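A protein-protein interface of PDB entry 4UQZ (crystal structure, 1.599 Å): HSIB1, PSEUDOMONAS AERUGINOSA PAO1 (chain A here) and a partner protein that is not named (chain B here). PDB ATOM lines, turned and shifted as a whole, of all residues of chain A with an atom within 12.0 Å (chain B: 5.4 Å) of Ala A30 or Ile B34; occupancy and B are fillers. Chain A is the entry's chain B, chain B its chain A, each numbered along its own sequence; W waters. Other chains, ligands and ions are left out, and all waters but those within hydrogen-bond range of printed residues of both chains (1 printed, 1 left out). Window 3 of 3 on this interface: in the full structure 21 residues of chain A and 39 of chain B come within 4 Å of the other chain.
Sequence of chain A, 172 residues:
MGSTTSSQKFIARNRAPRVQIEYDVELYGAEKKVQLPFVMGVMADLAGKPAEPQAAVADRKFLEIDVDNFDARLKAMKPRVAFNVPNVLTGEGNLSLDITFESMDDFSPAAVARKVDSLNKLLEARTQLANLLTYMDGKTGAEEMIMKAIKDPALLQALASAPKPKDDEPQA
The backbone NH (N) of Phe B35 sits close to the backbone carbonyl oxygen (O) of Leu A27 (3.4 Å). The side-chain amide nitrogen (NE2) of Gln B38 sits at hydrogen-bond distance from the backbone carbonyl oxygen (O) of Leu A27. The backbone carbonyl oxygen (O) of Gly A29 sits at hydrogen-bond distance from the guanidinium group (NH1) of Arg B183 (2.9 Å).
The side-chain amide nitrogen of Gln B38 sits close to the backbone carbonyl oxygen of Ile B34 (3.4 Å). OE1 of Gln B38 lies within hydrogen-bond range of N of Arg B183, 2.9 Å away.
Among the printed residues, pairs that only touch across the chains: Tyr A28 with Thr B31 (3.4 Å), Gly A29 with Ile B34 (3.5 Å), Ala A30 with Met B66 (3.6 Å), Ala A30 with Ile B34 (3.6 Å), Tyr A28 with Phe B35 (3.7 Å), Tyr A28 with Ile B34 (3.8 Å), Ala A30 with Arg B183 (3.8 Å) and Leu A27 with Ile B34 (3.9 Å).
Glu A26 touches none of the printed residues of chain B. Printed residues of chain B within 4 Å of Leu A27: Ile B34 (3.9 Å), Phe B35 (3.2 Å) and Gln B38 (3.0 Å). Printed residues of chain B within 4 Å of Tyr A28: Thr B31 (3.4 Å), Ile B34 (3.8 Å) and Phe B35 (3.7 Å). Of the printed residues of chain B, Gly A29 touches Ile B34 (3.5 Å) and Arg B183 (2.9 Å). Ala A30 touches three residues of chain B. Glu A31 touches none of the printed residues of chain B. Ala B30 touches none of the printed residues of chain A. Thr B31 touches one residue of chain A. Ile B34 touches just these residues of chain A: Leu A27, Tyr A28, Gly A29 and Ala A30. Leu B36 touches none of the printed residues of chain A. No residue of chain A comes within 4 Å of Phe B37. Gln B38 touches just one residue of chain A: Leu A27 (3.0 Å). No residue of chain A comes within 4 Å of Ala B63. Met B66 touches just one residue of chain A: Ala A30. Printed residues of chain A within 4 Å of Arg B183: Gly A29 (2.9 Å) and Ala A30 (3.8 Å). The nearest printed residue of chain B that does not touch Tyr A28 is Leu B32 (4.3 Å).
Of the 15 printed residues of chain B, 6 touch a printed residue of chain A. Of the 7 printed residues of chain A, 4 touch a printed residue of chain B. Printed residues of chain A that touch a printed residue of chain B: Leu A27, Tyr A28, Gly A29 and Ala A30.
Water W1 lies within hydrogen-bond range of NH2 of Arg B183, N of Glu A31 and O of Gly A29.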
ATOM      1  N   VAL A  25     -12.800  19.354  23.640  1.00  0.00           N
ATOM      2  CA  VAL A  25     -12.818  20.752  23.285  1.00  0.00           C
ATOM      3  C   VAL A  25     -12.276  20.922  21.886  1.00  0.00           C
ATOM      4  O   VAL A  25     -11.550  20.051  21.380  1.00  0.00           O
ATOM      5  CB  VAL A  25     -11.991  21.610  24.269  1.00  0.00           C
ATOM      6  CG1 VAL A  25     -12.648  21.597  25.630  1.00  0.00           C
ATOM      7  CG2 VAL A  25     -10.590  21.074  24.377  1.00  0.00           C
ATOM      8  N   GLU A  26     -12.683  22.014  21.254  1.00  0.00           N
ATOM      9  CA  GLU A  26     -12.198  22.356  19.919  1.00  0.00           C
ATOM     10  C   GLU A  26     -10.804  22.943  19.975  1.00  0.00           C
ATOM     11  O   GLU A  26     -10.428  23.609  20.934  1.00  0.00           O
ATOM     12  CB  GLU A  26     -13.155  23.321  19.227  1.00  0.00           C
ATOM     13  CG  GLU A  26     -14.565  22.774  19.128  1.00  0.00           C
ATOM     14  CD  GLU A  26     -15.016  22.470  17.720  1.00  0.00           C
ATOM     15  OE1 GLU A  26     -14.165  22.367  16.802  1.00  0.00           O
ATOM     16  OE2 GLU A  26     -16.245  22.330  17.534  1.00  0.00           O
ATOM     17  N   LEU A  27     -10.035  22.701  18.920  1.00  0.00           N
ATOM     18  CA  LEU A  27      -8.627  23.067  18.923  1.00  0.00           C
ATOM     19  C   LEU A  27      -8.290  24.159  17.926  1.00  0.00           C
ATOM     20  O   LEU A  27      -7.275  24.830  18.073  1.00  0.00           O
ATOM     21  CB  LEU A  27      -7.761  21.840  18.585  1.00  0.00           C
ATOM     22  CG  LEU A  27      -8.071  20.615  19.443  1.00  0.00           C
ATOM     23  CD1 LEU A  27      -7.202  19.416  19.015  1.00  0.00           C
ATOM     24  CD2 LEU A  27      -7.899  20.948  20.911  1.00  0.00           C
ATOM     25  N   TYR A  28      -9.121  24.318  16.900  1.00  0.00           N
ATOM     26  CA  TYR A  28      -8.727  25.154  15.772  1.00  0.00           C
ATOM     27  C   TYR A  28      -9.510  26.448  15.571  1.00  0.00           C
ATOM     28  O   TYR A  28      -9.191  27.209  14.659  1.00  0.00           O
ATOM     29  CB  TYR A  28      -8.802  24.322  14.481  1.00  0.00           C
ATOM     30  CG  TYR A  28      -7.960  23.080  14.547  1.00  0.00           C
ATOM     31  CD1 TYR A  28      -6.583  23.165  14.581  1.00  0.00           C
ATOM     32  CD2 TYR A  28      -8.547  21.814  14.564  1.00  0.00           C
ATOM     33  CE1 TYR A  28      -5.803  22.041  14.639  1.00  0.00           C
ATOM     34  CE2 TYR A  28      -7.772  20.666  14.628  1.00  0.00           C
ATOM     35  CZ  TYR A  28      -6.401  20.787  14.662  1.00  0.00           C
ATOM     36  OH  TYR A  28      -5.604  19.673  14.724  1.00  0.00           O
ATOM     37  N   GLY A  29     -10.487  26.723  16.425  1.00  0.00           N
ATOM     38  CA  GLY A  29     -11.372  27.859  16.209  1.00  0.00           C
ATOM     39  C   GLY A  29     -10.956  29.135  16.917  1.00  0.00           C
ATOM     40  O   GLY A  29     -10.381  29.081  17.988  1.00  0.00           O
ATOM     41  N   ALA A  30     -11.245  30.287  16.313  1.00  0.00           N
ATOM     42  CA  ALA A  30     -10.917  31.563  16.947  1.00  0.00           C
ATOM     43  C   ALA A  30     -12.105  32.522  16.993  1.00  0.00           C
ATOM     44  O   ALA A  30     -11.916  33.738  17.062  1.00  0.00           O
ATOM     45  CB  ALA A  30      -9.733  32.233  16.223  1.00  0.00           C
ATOM     46  N   GLU A  31     -13.318  31.995  16.932  1.00  0.00           N
ATOM     47  CA  GLU A  31     -14.500  32.843  17.094  1.00  0.00           C
ATOM     48  C   GLU A  31     -15.567  32.147  17.944  1.00  0.00           C
ATOM     49  O   GLU A  31     -16.124  32.734  18.881  1.00  0.00           O
ATOM     50  CB  GLU A  31     -15.067  33.238  15.732  1.00  0.00           C
ATOM     51  N   ALA B  30      -2.823  29.142   9.835  1.00  0.00           N
ATOM     52  CA  ALA B  30      -3.247  29.841  11.030  1.00  0.00           C
ATOM     53  C   ALA B  30      -3.912  28.911  12.024  1.00  0.00           C
ATOM     54  O   ALA B  30      -3.815  29.154  13.223  1.00  0.00           O
ATOM     55  CB  ALA B  30      -4.197  30.973  10.690  1.00  0.00           C
ATOM     56  N   THR B  31      -4.590  27.878  11.541  1.00  0.00           N
ATOM     57  CA  THR B  31      -5.354  27.037  12.475  1.00  0.00           C
ATOM     58  C   THR B  31      -4.412  26.225  13.354  1.00  0.00           C
ATOM     59  O   THR B  31      -4.682  26.009  14.537  1.00  0.00           O
ATOM     60  CB  THR B  31      -6.347  26.093  11.773  1.00  0.00           C
ATOM     61  OG1 THR B  31      -5.649  25.039  11.097  1.00  0.00           O
ATOM     62  CG2 THR B  31      -7.234  26.847  10.805  1.00  0.00           C
ATOM     63  N   LEU B  32      -3.290  25.791  12.806  1.00  0.00           N
ATOM     64  CA  LEU B  32      -2.322  25.064  13.613  1.00  0.00           C
ATOM     65  C   LEU B  32      -1.755  25.967  14.685  1.00  0.00           C
ATOM     66  O   LEU B  32      -1.414  25.510  15.772  1.00  0.00           O
ATOM     67  CB  LEU B  32      -1.176  24.506  12.765  1.00  0.00           C
ATOM     68  CG  LEU B  32      -1.578  23.603  11.614  1.00  0.00           C
ATOM     69  CD1 LEU B  32      -0.336  23.235  10.785  1.00  0.00           C
ATOM     70  CD2 LEU B  32      -2.282  22.372  12.168  1.00  0.00           C
ATOM     71  N   ARG B  33      -1.606  27.256  14.371  1.00  0.00           N
ATOM     72  CA  ARG B  33      -1.037  28.178  15.342  1.00  0.00           C
ATOM     73  C   ARG B  33      -2.058  28.563  16.390  1.00  0.00           C
ATOM     74  O   ARG B  33      -1.695  28.909  17.499  1.00  0.00           O
ATOM     75  CB  ARG B  33      -0.484  29.408  14.647  1.00  0.00           C
ATOM     76  CG  ARG B  33       0.728  29.061  13.826  1.00  0.00           C
ATOM     77  CD  ARG B  33       1.417  30.298  13.292  1.00  0.00           C
ATOM     78  NE  ARG B  33       2.510  30.002  12.374  1.00  0.00           N
ATOM     79  CZ  ARG B  33       3.795  29.865  12.718  1.00  0.00           C
ATOM     80  NH1 ARG B  33       4.126  30.007  14.001  1.00  0.00           N
ATOM     81  NH2 ARG B  33       4.740  29.591  11.776  1.00  0.00           N
ATOM     82  N   ILE B  34      -3.334  28.516  16.028  1.00  0.00           N
ATOM     83  CA  ILE B  34      -4.409  28.677  17.012  1.00  0.00           C
ATOM     84  C   ILE B  34      -4.408  27.515  18.017  1.00  0.00           C
ATOM     85  O   ILE B  34      -4.425  27.733  19.233  1.00  0.00           O
ATOM     86  CB  ILE B  34      -5.775  28.805  16.311  1.00  0.00           C
ATOM     87  CG1 ILE B  34      -5.855  30.172  15.619  1.00  0.00           C
ATOM     88  CG2 ILE B  34      -6.944  28.657  17.300  1.00  0.00           C
ATOM     89  CD1 ILE B  34      -7.044  30.319  14.683  1.00  0.00           C
ATOM     90  N   PHE B  35      -4.303  26.285  17.507  1.00  0.00           N
ATOM     91  CA  PHE B  35      -4.143  25.118  18.381  1.00  0.00           C
ATOM     92  C   PHE B  35      -2.890  25.354  19.272  1.00  0.00           C
ATOM     93  O   PHE B  35      -2.965  25.202  20.486  1.00  0.00           O
ATOM     94  CB  PHE B  35      -4.057  23.856  17.517  1.00  0.00           C
ATOM     95  CG  PHE B  35      -3.848  22.547  18.266  1.00  0.00           C
ATOM     96  CD1 PHE B  35      -4.000  22.441  19.641  1.00  0.00           C
ATOM     97  CD2 PHE B  35      -3.548  21.401  17.545  1.00  0.00           C
ATOM     98  CE1 PHE B  35      -3.810  21.230  20.275  1.00  0.00           C
ATOM     99  CE2 PHE B  35      -3.370  20.174  18.176  1.00  0.00           C
ATOM    100  CZ  PHE B  35      -3.482  20.089  19.540  1.00  0.00           C
ATOM    101  N   LEU B  36      -1.767  25.744  18.672  1.00  0.00           N
ATOM    102  CA  LEU B  36      -0.508  25.837  19.396  1.00  0.00           C
ATOM    103  C   LEU B  36      -0.562  26.896  20.512  1.00  0.00           C
ATOM    104  O   LEU B  36      -0.072  26.681  21.636  1.00  0.00           O
ATOM    105  CB  LEU B  36       0.633  26.153  18.414  1.00  0.00           C
ATOM    106  CG  LEU B  36       2.045  26.205  18.995  1.00  0.00           C
ATOM    107  CD1 LEU B  36       2.365  24.963  19.771  1.00  0.00           C
ATOM    108  CD2 LEU B  36       3.092  26.408  17.865  1.00  0.00           C
ATOM    109  N   PHE B  37      -1.154  28.052  20.215  1.00  0.00           N
ATOM    110  CA  PHE B  37      -1.269  29.078  21.241  1.00  0.00           C
ATOM    111  C   PHE B  37      -2.054  28.527  22.437  1.00  0.00           C
ATOM    112  O   PHE B  37      -1.666  28.734  23.588  1.00  0.00           O
ATOM    113  CB  PHE B  37      -1.927  30.359  20.675  1.00  0.00           C
ATOM    114  CG  PHE B  37      -3.064  30.883  21.483  1.00  0.00           C
ATOM    115  CD1 PHE B  37      -2.866  31.438  22.758  1.00  0.00           C
ATOM    116  CD2 PHE B  37      -4.357  30.840  20.985  1.00  0.00           C
ATOM    117  CE1 PHE B  37      -3.935  31.892  23.491  1.00  0.00           C
ATOM    118  CE2 PHE B  37      -5.425  31.334  21.722  1.00  0.00           C
ATOM    119  CZ  PHE B  37      -5.222  31.842  22.979  1.00  0.00           C
ATOM    120  N   GLN B  38      -3.136  27.818  22.152  1.00  0.00           N
ATOM    121  CA  GLN B  38      -4.011  27.320  23.216  1.00  0.00           C
ATOM    122  C   GLN B  38      -3.280  26.247  24.007  1.00  0.00           C
ATOM    123  O   GLN B  38      -3.404  26.155  25.232  1.00  0.00           O
ATOM    124  CB  GLN B  38      -5.298  26.782  22.611  1.00  0.00           C
ATOM    125  CG  GLN B  38      -6.132  27.892  21.994  1.00  0.00           C
ATOM    126  CD  GLN B  38      -7.477  27.426  21.546  1.00  0.00           C
ATOM    127  OE1 GLN B  38      -8.486  27.645  22.205  1.00  0.00           O
ATOM    128  NE2 GLN B  38      -7.514  26.765  20.398  1.00  0.00           N
ATOM    129  N   LEU B  39      -2.540  25.398  23.298  1.00  0.00           N
ATOM    130  CA  LEU B  39      -1.799  24.350  23.987  1.00  0.00           C
ATOM    131  C   LEU B  39      -0.700  24.904  24.857  1.00  0.00           C
ATOM    132  O   LEU B  39      -0.532  24.482  26.001  1.00  0.00           O
ATOM    133  CB  LEU B  39      -1.242  23.349  22.975  1.00  0.00           C
ATOM    134  CG  LEU B  39      -0.463  22.163  23.554  1.00  0.00           C
ATOM    135  CD1 LEU B  39      -1.375  21.313  24.454  1.00  0.00           C
ATOM    136  CD2 LEU B  39       0.133  21.290  22.416  1.00  0.00           C
ATOM    137  N   VAL B  56      -0.577  34.483  14.571  1.00  0.00           N
ATOM    138  CA  VAL B  56      -1.946  34.284  14.145  1.00  0.00           C
ATOM    139  C   VAL B  56      -2.564  35.593  13.646  1.00  0.00           C
ATOM    140  O   VAL B  56      -3.195  35.618  12.577  1.00  0.00           O
ATOM    141  CB  VAL B  56      -2.778  33.700  15.266  1.00  0.00           C
ATOM    142  CG1 VAL B  56      -4.237  33.699  14.890  1.00  0.00           C
ATOM    143  CG2 VAL B  56      -2.290  32.294  15.521  1.00  0.00           C
ATOM    144  N   ASP B  60      -3.987  35.874   9.885  1.00  0.00           N
ATOM    145  CA  ASP B  60      -5.439  35.881   9.783  1.00  0.00           C
ATOM    146  C   ASP B  60      -5.980  37.076  10.549  1.00  0.00           C
ATOM    147  O   ASP B  60      -6.168  37.002  11.768  1.00  0.00           O
ATOM    148  CB  ASP B  60      -6.015  34.570  10.333  1.00  0.00           C
ATOM    149  CG  ASP B  60      -7.529  34.487  10.212  1.00  0.00           C
ATOM    150  OD1 ASP B  60      -8.127  35.360   9.549  1.00  0.00           O
ATOM    151  OD2 ASP B  60      -8.120  33.539  10.784  1.00  0.00           O
ATOM    152  N   ALA B  63      -8.845  37.050  13.108  1.00  0.00           N
ATOM    153  CA  ALA B  63      -8.581  36.527  14.451  1.00  0.00           C
ATOM    154  C   ALA B  63      -8.063  37.587  15.431  1.00  0.00           C
ATOM    155  O   ALA B  63      -7.831  37.286  16.613  1.00  0.00           O
ATOM    156  CB  ALA B  63      -7.596  35.394  14.372  1.00  0.00           C
ATOM    157  N   MET B  66      -9.682  38.047  18.968  1.00  0.00           N
ATOM    158  CA  MET B  66      -9.187  36.998  19.862  1.00  0.00           C
ATOM    159  C   MET B  66      -7.762  37.293  20.319  1.00  0.00           C
ATOM    160  O   MET B  66      -7.440  37.125  21.512  1.00  0.00           O
ATOM    161  CB  MET B  66      -9.230  35.599  19.225  1.00  0.00           C
ATOM    162  CG  MET B  66      -8.529  34.528  20.105  1.00  0.00           C
ATOM    163  SD  MET B  66      -8.474  32.824  19.503  1.00  0.00           S
ATOM    164  CE  MET B  66      -6.971  32.905  18.527  1.00  0.00           C
ATOM    165  N   ARG B 183      -8.786  26.907  24.951  1.00  0.00           N
ATOM    166  CA  ARG B 183      -8.401  28.046  25.798  1.00  0.00           C
ATOM    167  C   ARG B 183      -9.375  28.172  26.946  1.00  0.00           C
ATOM    168  O   ARG B 183      -9.024  28.769  27.965  1.00  0.00           O
ATOM    169  CB  ARG B 183      -8.323  29.361  24.997  1.00  0.00           C
ATOM    170  CG  ARG B 183      -9.599  29.707  24.315  1.00  0.00           C
ATOM    171  CD  ARG B 183      -9.319  30.797  23.297  1.00  0.00           C
ATOM    172  NE  ARG B 183     -10.454  31.190  22.485  1.00  0.00           N
ATOM    173  CZ  ARG B 183     -10.796  30.644  21.328  1.00  0.00           C
ATOM    174  NH1 ARG B 183     -10.149  29.569  20.871  1.00  0.00           N
ATOM    175  NH2 ARG B 183     -11.813  31.158  20.629  1.00  0.00           N
HETATM  176  O   HOH W   1     -13.598  29.886  19.008  1.00  0.00           O
